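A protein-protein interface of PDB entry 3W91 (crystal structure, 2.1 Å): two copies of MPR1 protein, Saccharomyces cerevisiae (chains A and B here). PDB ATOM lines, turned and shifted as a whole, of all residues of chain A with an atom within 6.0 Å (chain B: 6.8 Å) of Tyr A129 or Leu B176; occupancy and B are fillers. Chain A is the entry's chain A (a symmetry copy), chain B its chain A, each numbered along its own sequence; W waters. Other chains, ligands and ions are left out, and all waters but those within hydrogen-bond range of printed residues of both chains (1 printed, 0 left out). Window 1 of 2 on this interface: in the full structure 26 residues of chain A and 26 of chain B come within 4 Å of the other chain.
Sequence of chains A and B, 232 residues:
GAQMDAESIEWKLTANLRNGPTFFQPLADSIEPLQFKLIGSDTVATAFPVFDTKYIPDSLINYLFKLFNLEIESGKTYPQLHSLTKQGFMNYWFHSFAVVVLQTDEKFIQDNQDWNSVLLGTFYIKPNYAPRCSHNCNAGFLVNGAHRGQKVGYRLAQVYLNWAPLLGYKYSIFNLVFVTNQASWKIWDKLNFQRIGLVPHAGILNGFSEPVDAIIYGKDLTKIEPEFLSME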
ATOM      1  N   PRO A 127       4.527  23.562   8.779  1.00  0.00           N
ATOM      2  CA  PRO A 127       5.628  23.686   9.754  1.00  0.00           C
ATOM      3  C   PRO A 127       5.979  22.298  10.301  1.00  0.00           C
ATOM      4  O   PRO A 127       5.080  21.530  10.623  1.00  0.00           O
ATOM      5  CB  PRO A 127       5.018  24.531  10.862  1.00  0.00           C
ATOM      6  CG  PRO A 127       3.912  25.306  10.180  1.00  0.00           C
ATOM      7  CD  PRO A 127       3.327  24.306   9.200  1.00  0.00           C
ATOM      8  N   ASN A 128       7.264  21.967  10.385  1.00  0.00           N
ATOM      9  CA  ASN A 128       7.643  20.640  10.886  1.00  0.00           C
ATOM     10  C   ASN A 128       7.599  20.577  12.404  1.00  0.00           C
ATOM     11  O   ASN A 128       7.614  19.493  12.975  1.00  0.00           O
ATOM     12  CB  ASN A 128       9.037  20.245  10.388  1.00  0.00           C
ATOM     13  CG  ASN A 128       9.322  18.748  10.542  1.00  0.00           C
ATOM     14  OD1 ASN A 128       8.538  17.898  10.095  1.00  0.00           O
ATOM     15  ND2 ASN A 128      10.426  18.422  11.222  1.00  0.00           N
ATOM     16  N   TYR A 129       7.568  21.741  13.059  1.00  0.00           N
ATOM     17  CA  TYR A 129       7.648  21.780  14.501  1.00  0.00           C
ATOM     18  C   TYR A 129       6.716  22.836  15.057  1.00  0.00           C
ATOM     19  O   TYR A 129       6.224  23.694  14.315  1.00  0.00           O
ATOM     20  CB  TYR A 129       9.034  22.200  14.938  1.00  0.00           C
ATOM     21  CG  TYR A 129      10.211  21.393  14.397  1.00  0.00           C
ATOM     22  CD1 TYR A 129      10.549  20.149  14.937  1.00  0.00           C
ATOM     23  CD2 TYR A 129      11.015  21.921  13.392  1.00  0.00           C
ATOM     24  CE1 TYR A 129      11.659  19.437  14.464  1.00  0.00           C
ATOM     25  CE2 TYR A 129      12.111  21.231  12.913  1.00  0.00           C
ATOM     26  CZ  TYR A 129      12.439  19.993  13.452  1.00  0.00           C
ATOM     27  OH  TYR A 129      13.545  19.332  12.939  1.00  0.00           O
ATOM     28  N   ALA A 130       6.581  22.826  16.385  1.00  0.00           N
ATOM     29  CA  ALA A 130       5.865  23.859  17.114  1.00  0.00           C
ATOM     30  C   ALA A 130       6.511  25.238  16.904  1.00  0.00           C
ATOM     31  O   ALA A 130       7.619  25.332  16.358  1.00  0.00           O
ATOM     32  CB  ALA A 130       5.777  23.482  18.603  1.00  0.00           C
ATOM     33  N   PRO A 131       5.826  26.317  17.339  1.00  0.00           N
ATOM     34  CA  PRO A 131       6.079  27.679  16.841  1.00  0.00           C
ATOM     35  C   PRO A 131       7.516  28.251  16.831  1.00  0.00           C
ATOM     36  O   PRO A 131       7.893  28.869  15.846  1.00  0.00           O
ATOM     37  CB  PRO A 131       5.091  28.538  17.637  1.00  0.00           C
ATOM     38  CG  PRO A 131       3.924  27.589  17.834  1.00  0.00           C
ATOM     39  CD  PRO A 131       4.602  26.268  18.164  1.00  0.00           C
ATOM     40  N   CYS A 133      10.181  26.819  16.298  1.00  0.00           N
ATOM     41  CA  CYS A 133      10.902  26.177  15.197  1.00  0.00           C
ATOM     42  C   CYS A 133      10.057  26.031  13.920  1.00  0.00           C
ATOM     43  O   CYS A 133      10.364  25.224  13.033  1.00  0.00           O
ATOM     44  CB  CYS A 133      11.427  24.806  15.665  1.00  0.00           C
ATOM     45  SG  CYS A 133      12.451  24.912  17.157  1.00  0.00           S
ATOM     46  N   SER A 134       9.006  26.840  13.817  1.00  0.00           N
ATOM     47  CA  SER A 134       8.027  26.703  12.734  1.00  0.00           C
ATOM     48  C   SER A 134       8.499  27.281  11.405  1.00  0.00           C
ATOM     49  O   SER A 134       7.809  27.130  10.402  1.00  0.00           O
ATOM     50  CB  SER A 134       6.702  27.348  13.130  1.00  0.00           C
ATOM     51  OG  SER A 134       6.928  28.718  13.403  1.00  0.00           O
ATOM     52  N   ASN A 136      10.935  26.002   9.977  1.00  0.00           N
ATOM     53  CA  ASN A 136      11.305  24.760   9.301  1.00  0.00           C
ATOM     54  C   ASN A 136      10.047  24.057   8.805  1.00  0.00           C
ATOM     55  O   ASN A 136       9.209  23.658   9.612  1.00  0.00           O
ATOM     56  CB  ASN A 136      12.008  23.802  10.259  1.00  0.00           C
ATOM     57  CG  ASN A 136      13.272  24.371  10.827  1.00  0.00           C
ATOM     58  OD1 ASN A 136      14.339  24.273  10.202  1.00  0.00           O
ATOM     59  ND2 ASN A 136      13.184  24.936  12.035  1.00  0.00           N
ATOM     60  N   ILE A 173      12.861  20.372   6.311  1.00  0.00           N
ATOM     61  CA  ILE A 173      13.213  19.111   6.975  1.00  0.00           C
ATOM     62  C   ILE A 173      12.285  18.011   6.507  1.00  0.00           C
ATOM     63  O   ILE A 173      11.042  18.169   6.587  1.00  0.00           O
ATOM     64  CB  ILE A 173      13.011  19.157   8.499  1.00  0.00           C
ATOM     65  CG1 ILE A 173      13.837  20.278   9.138  1.00  0.00           C
ATOM     66  CG2 ILE A 173      13.370  17.804   9.100  1.00  0.00           C
ATOM     67  CD1 ILE A 173      15.292  19.924   9.291  1.00  0.00           C
ATOM     68  N   ASN A 175      11.621  14.207   7.748  1.00  0.00           N
ATOM     69  CA  ASN A 175      11.990  13.385   8.923  1.00  0.00           C
ATOM     70  C   ASN A 175      12.322  11.942   8.604  1.00  0.00           C
ATOM     71  O   ASN A 175      13.125  11.337   9.284  1.00  0.00           O
ATOM     72  CB  ASN A 175      10.857  13.403   9.953  1.00  0.00           C
ATOM     73  CG  ASN A 175      10.417  14.802  10.267  1.00  0.00           C
ATOM     74  OD1 ASN A 175      11.176  15.575  10.859  1.00  0.00           O
ATOM     75  ND2 ASN A 175       9.205  15.167   9.818  1.00  0.00           N
ATOM     76  N   THR B  77      14.093  26.201  25.722  1.00  0.00           N
ATOM     77  CA  THR B  77      14.328  24.758  25.809  1.00  0.00           C
ATOM     78  C   THR B  77      13.314  23.939  24.995  1.00  0.00           C
ATOM     79  O   THR B  77      13.652  22.883  24.466  1.00  0.00           O
ATOM     80  CB  THR B  77      14.324  24.266  27.280  1.00  0.00           C
ATOM     81  OG1 THR B  77      13.074  24.602  27.873  1.00  0.00           O
ATOM     82  CG2 THR B  77      15.422  24.935  28.109  1.00  0.00           C
ATOM     83  N   TYR B  78      12.091  24.446  24.875  1.00  0.00           N
ATOM     84  CA  TYR B  78      11.034  23.779  24.087  1.00  0.00           C
ATOM     85  C   TYR B  78      10.600  24.656  22.906  1.00  0.00           C
ATOM     86  O   TYR B  78      10.751  25.877  22.954  1.00  0.00           O
ATOM     87  CB  TYR B  78       9.837  23.470  24.990  1.00  0.00           C
ATOM     88  CG  TYR B  78      10.028  22.257  25.876  1.00  0.00           C
ATOM     89  CD1 TYR B  78      10.787  22.328  27.055  1.00  0.00           C
ATOM     90  CD2 TYR B  78       9.469  21.023  25.525  1.00  0.00           C
ATOM     91  CE1 TYR B  78      10.978  21.209  27.862  1.00  0.00           C
ATOM     92  CE2 TYR B  78       9.639  19.907  26.341  1.00  0.00           C
ATOM     93  CZ  TYR B  78      10.403  20.007  27.492  1.00  0.00           C
ATOM     94  OH  TYR B  78      10.561  18.887  28.275  1.00  0.00           O
ATOM     95  N   PRO B  79      10.071  24.040  21.834  1.00  0.00           N
ATOM     96  CA  PRO B  79       9.641  24.824  20.669  1.00  0.00           C
ATOM     97  C   PRO B  79       8.266  25.480  20.885  1.00  0.00           C
ATOM     98  O   PRO B  79       7.903  26.431  20.184  1.00  0.00           O
ATOM     99  CB  PRO B  79       9.583  23.773  19.553  1.00  0.00           C
ATOM    100  CG  PRO B  79       9.222  22.491  20.266  1.00  0.00           C
ATOM    101  CD  PRO B  79       9.965  22.584  21.588  1.00  0.00           C
ATOM    102  N   ASN B 138      10.121   9.153  21.796  1.00  0.00           N
ATOM    103  CA  ASN B 138      10.575  10.480  22.136  1.00  0.00           C
ATOM    104  C   ASN B 138      10.411  10.625  23.646  1.00  0.00           C
ATOM    105  O   ASN B 138       9.598   9.925  24.253  1.00  0.00           O
ATOM    106  CB  ASN B 138       9.688  11.521  21.433  1.00  0.00           C
ATOM    107  CG  ASN B 138      10.145  12.942  21.696  1.00  0.00           C
ATOM    108  OD1 ASN B 138      11.335  13.271  21.511  1.00  0.00           O
ATOM    109  ND2 ASN B 138       9.219  13.795  22.125  1.00  0.00           N
ATOM    110  N   ILE B 173      14.728   8.807  20.061  1.00  0.00           N
ATOM    111  CA  ILE B 173      15.003  10.005  19.260  1.00  0.00           C
ATOM    112  C   ILE B 173      14.580  11.241  20.024  1.00  0.00           C
ATOM    113  O   ILE B 173      13.410  11.323  20.473  1.00  0.00           O
ATOM    114  CB  ILE B 173      14.183  10.061  17.960  1.00  0.00           C
ATOM    115  CG1 ILE B 173      14.439   8.833  17.082  1.00  0.00           C
ATOM    116  CG2 ILE B 173      14.507  11.347  17.208  1.00  0.00           C
ATOM    117  CD1 ILE B 173      15.738   8.912  16.324  1.00  0.00           C
ATOM    118  N   PHE B 174      15.507  12.185  20.196  1.00  0.00           N
ATOM    119  CA  PHE B 174      15.103  13.534  20.587  1.00  0.00           C
ATOM    120  C   PHE B 174      15.260  14.453  19.376  1.00  0.00           C
ATOM    121  O   PHE B 174      16.344  14.537  18.778  1.00  0.00           O
ATOM    122  CB  PHE B 174      15.928  14.083  21.762  1.00  0.00           C
ATOM    123  CG  PHE B 174      16.009  13.150  22.963  1.00  0.00           C
ATOM    124  CD1 PHE B 174      14.917  12.389  23.360  1.00  0.00           C
ATOM    125  CD2 PHE B 174      17.176  13.064  23.695  1.00  0.00           C
ATOM    126  CE1 PHE B 174      14.990  11.550  24.446  1.00  0.00           C
ATOM    127  CE2 PHE B 174      17.265  12.222  24.790  1.00  0.00           C
ATOM    128  CZ  PHE B 174      16.159  11.477  25.172  1.00  0.00           C
ATOM    129  N   ASN B 175      14.192  15.149  19.014  1.00  0.00           N
ATOM    130  CA  ASN B 175      14.187  15.935  17.759  1.00  0.00           C
ATOM    131  C   ASN B 175      14.886  17.275  17.851  1.00  0.00           C
ATOM    132  O   ASN B 175      15.433  17.746  16.875  1.00  0.00           O
ATOM    133  CB  ASN B 175      12.747  16.174  17.294  1.00  0.00           C
ATOM    134  CG  ASN B 175      11.960  14.897  17.250  1.00  0.00           C
ATOM    135  OD1 ASN B 175      12.246  14.021  16.429  1.00  0.00           O
ATOM    136  ND2 ASN B 175      11.001  14.750  18.177  1.00  0.00           N
ATOM    137  N   LEU B 176      14.814  17.902  19.020  1.00  0.00           N
ATOM    138  CA  LEU B 176      15.275  19.278  19.183  1.00  0.00           C
ATOM    139  C   LEU B 176      15.949  19.500  20.528  1.00  0.00           C
ATOM    140  O   LEU B 176      15.344  20.044  21.446  1.00  0.00           O
ATOM    141  CB  LEU B 176      14.081  20.246  19.084  1.00  0.00           C
ATOM    142  CG  LEU B 176      13.382  20.364  17.730  1.00  0.00           C
ATOM    143  CD1 LEU B 176      11.981  20.946  17.893  1.00  0.00           C
ATOM    144  CD2 LEU B 176      14.211  21.199  16.767  1.00  0.00           C
ATOM    145  N   VAL B 177      17.195  19.100  20.670  1.00  0.00           N
ATOM    146  CA  VAL B 177      17.919  19.525  21.844  1.00  0.00           C
ATOM    147  C   VAL B 177      18.788  20.722  21.447  1.00  0.00           C
ATOM    148  O   VAL B 177      19.802  20.575  20.777  1.00  0.00           O
ATOM    149  CB  VAL B 177      18.700  18.381  22.489  1.00  0.00           C
ATOM    150  CG1 VAL B 177      19.435  18.881  23.720  1.00  0.00           C
ATOM    151  CG2 VAL B 177      17.739  17.255  22.872  1.00  0.00           C
ATOM    152  N   PHE B 178      18.348  21.925  21.812  1.00  0.00           N
ATOM    153  CA  PHE B 178      19.075  23.123  21.409  1.00  0.00           C
ATOM    154  C   PHE B 178      20.502  23.064  21.942  1.00  0.00           C
ATOM    155  O   PHE B 178      20.736  22.513  23.018  1.00  0.00           O
ATOM    156  CB  PHE B 178      18.343  24.373  21.870  1.00  0.00           C
ATOM    157  CG  PHE B 178      16.976  24.507  21.249  1.00  0.00           C
ATOM    158  CD1 PHE B 178      16.847  24.712  19.875  1.00  0.00           C
ATOM    159  CD2 PHE B 178      15.832  24.373  22.019  1.00  0.00           C
ATOM    160  CE1 PHE B 178      15.587  24.796  19.283  1.00  0.00           C
ATOM    161  CE2 PHE B 178      14.573  24.450  21.430  1.00  0.00           C
ATOM    162  CZ  PHE B 178      14.457  24.665  20.065  1.00  0.00           C
ATOM    163  N   ASN B 181      21.173  24.247  25.318  1.00  0.00           N
ATOM    164  CA  ASN B 181      20.690  23.455  26.445  1.00  0.00           C
ATOM    165  C   ASN B 181      21.838  22.597  27.012  1.00  0.00           C
ATOM    166  O   ASN B 181      22.356  21.692  26.348  1.00  0.00           O
ATOM    167  CB  ASN B 181      19.499  22.598  26.012  1.00  0.00           C
ATOM    168  CG  ASN B 181      18.791  21.931  27.183  1.00  0.00           C
ATOM    169  OD1 ASN B 181      19.349  21.785  28.266  1.00  0.00           O
ATOM    170  ND2 ASN B 181      17.546  21.531  26.965  1.00  0.00           N
ATOM    171  N   VAL B 199      20.166  20.331  13.184  1.00  0.00           N
ATOM    172  CA  VAL B 199      19.361  21.303  12.424  1.00  0.00           C
ATOM    173  C   VAL B 199      19.915  22.715  12.625  1.00  0.00           C
ATOM    174  O   VAL B 199      19.817  23.260  13.719  1.00  0.00           O
ATOM    175  CB  VAL B 199      17.903  21.276  12.903  1.00  0.00           C
ATOM    176  CG1 VAL B 199      17.048  22.228  12.076  1.00  0.00           C
ATOM    177  CG2 VAL B 199      17.369  19.851  12.843  1.00  0.00           C
ATOM    178  N   ALA B 202      17.789  26.122  13.954  1.00  0.00           N
ATOM    179  CA  ALA B 202      16.499  25.471  14.202  1.00  0.00           C
ATOM    180  C   ALA B 202      15.440  26.312  14.920  1.00  0.00           C
ATOM    181  O   ALA B 202      14.266  26.234  14.580  1.00  0.00           O
ATOM    182  CB  ALA B 202      16.723  24.194  14.974  1.00  0.00           C
ATOM    183  N   GLY B 203      15.854  27.066  15.935  1.00  0.00           N
ATOM    184  CA  GLY B 203      14.922  27.679  16.875  1.00  0.00           C
ATOM    185  C   GLY B 203      15.111  29.164  17.149  1.00  0.00           C
ATOM    186  O   GLY B 203      16.240  29.650  17.300  1.00  0.00           O
ATOM    187  N   ALA B 214      19.879  23.051  16.730  1.00  0.00           N
ATOM    188  CA  ALA B 214      19.414  21.971  17.593  1.00  0.00           C
ATOM    189  C   ALA B 214      20.011  20.626  17.211  1.00  0.00           C
ATOM    190  O   ALA B 214      20.150  20.295  16.027  1.00  0.00           O
ATOM    191  CB  ALA B 214      17.878  21.893  17.624  1.00  0.00           C
ATOM    192  N   ILE B 215      20.364  19.846  18.228  1.00  0.00           N
ATOM    193  CA  ILE B 215      20.876  18.501  18.006  1.00  0.00           C
ATOM    194  C   ILE B 215      19.743  17.452  17.951  1.00  0.00           C
ATOM    195  O   ILE B 215      18.787  17.520  18.731  1.00  0.00           O
ATOM    196  CB  ILE B 215      21.865  18.102  19.121  1.00  0.00           C
ATOM    197  CG1 ILE B 215      23.010  19.125  19.214  1.00  0.00           C
ATOM    198  CG2 ILE B 215      22.405  16.700  18.878  1.00  0.00           C
ATOM    199  CD1 ILE B 215      23.597  19.251  20.606  1.00  0.00           C
ATOM    200  N   ILE B 216      19.852  16.521  17.010  1.00  0.00           N
ATOM    201  CA  ILE B 216      18.972  15.358  16.956  1.00  0.00           C
ATOM    202  C   ILE B 216      19.749  14.216  17.593  1.00  0.00           C
ATOM    203  O   ILE B 216      20.826  13.842  17.114  1.00  0.00           O
ATOM    204  CB  ILE B 216      18.590  14.981  15.510  1.00  0.00           C
ATOM    205  CG1 ILE B 216      17.903  16.178  14.826  1.00  0.00           C
ATOM    206  CG2 ILE B 216      17.653  13.780  15.518  1.00  0.00           C
ATOM    207  CD1 ILE B 216      17.736  16.058  13.319  1.00  0.00           C
ATOM    208  N   TYR B 217      19.245  13.726  18.724  1.00  0.00           N
ATOM    209  CA  TYR B 217      19.922  12.654  19.452  1.00  0.00           C
ATOM    210  C   TYR B 217      19.241  11.316  19.205  1.00  0.00           C
ATOM    211  O   TYR B 217      18.010  11.229  19.206  1.00  0.00           O
ATOM    212  CB  TYR B 217      19.873  12.933  20.947  1.00  0.00           C
ATOM    213  CG  TYR B 217      20.977  13.809  21.451  1.00  0.00           C
ATOM    214  CD1 TYR B 217      22.263  13.323  21.576  1.00  0.00           C
ATOM    215  CD2 TYR B 217      20.731  15.120  21.841  1.00  0.00           C
ATOM    216  CE1 TYR B 217      23.285  14.122  22.042  1.00  0.00           C
ATOM    217  CE2 TYR B 217      21.757  15.931  22.312  1.00  0.00           C
ATOM    218  CZ  TYR B 217      23.024  15.420  22.421  1.00  0.00           C
ATOM    219  OH  TYR B 217      24.060  16.216  22.897  1.00  0.00           O
HETATM  220  O   HOH W   1      14.373  17.212  14.240  1.00  0.00           O
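Tyr A129 touches just these residues of chain B: Leu B176 and Val B199.
Leu B176 touches just one residue of chain A: Tyr A129.
Printed residues of chain B within 4 Å of Cys A133: Pro B79 (3.9 Å), Phe B178 (3.5 Å), Ala B202 (3.4 Å) and Gly B203 (3.7 Å).
Of the printed residues of chain A, Ala B202 touches Cys A133 (3.4 Å) and Asn A136 (3.1 Å).
Printed residues of chain A within 4 Å of Pro B79: Ala A130 (3.8 Å), Pro A131 (3.5 Å) and Cys A133 (3.9 Å).
Of the printed residues of chain A, Val B199 touches Tyr A129 (3.9 Å) and Asn A136 (3.9 Å).
Tyr B78 touches none of the printed residues of chain A.
Positions printed for both chains: 173 and 175.
Of the 10 pairs that touch across the chains among the printed residues, none has its exchanged pair printed and touching as well.
Of the 18 printed residues of chain B, 6 touch a printed residue of chain A.
Printed residues of chain B that touch a printed residue of chain A: Pro B79, Leu B176, Phe B178, Val B199, Ala B202 and Gly B203.
Hydrophobic or aromatic side chains of chain A that line the printed part of chain B: Tyr A129, Ala A130 and Pro A131.
N of Val B199 is in hydrogen-bond range of O of Ala B214 (2.8 Å).
O of Asn A136 lies within hydrogen-bond range of N of Asn A128, 2.7 Å away.
The side-chain hydroxyl (OG) of Ser A134 sits at hydrogen-bond distance from the backbone carbonyl oxygen (O) of Pro A131.
The side-chain amide nitrogen of Asn A136 is in hydrogen-bond range of the backbone carbonyl oxygen of Cys A133.
Among the printed residues, pairs that only touch across the chains: Tyr A129 with Leu B176 (3.4 Å), Pro A131 with Pro B79 (3.5 Å), Cys A133 with Phe B178 (3.5 Å), Cys A133 with Gly B203 (3.7 Å), Ala A130 with Pro B79 (3.8 Å), Tyr A129 with Val B199 (3.9 Å), Asn A136 with Val B199 (3.9 Å) and Cys A133 with Pro B79 (3.9 Å).
Water W1 lies within hydrogen-bond range of OH of Tyr A129 and O of Asn B175.
SG of Cys A133 sits close to O of Ala B202, 3.4 Å away.
The side-chain amide nitrogen (ND2) of Asn A136 sits at hydrogen-bond distance from the backbone carbonyl oxygen (O) of Ala B202, 3.1 Å away.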
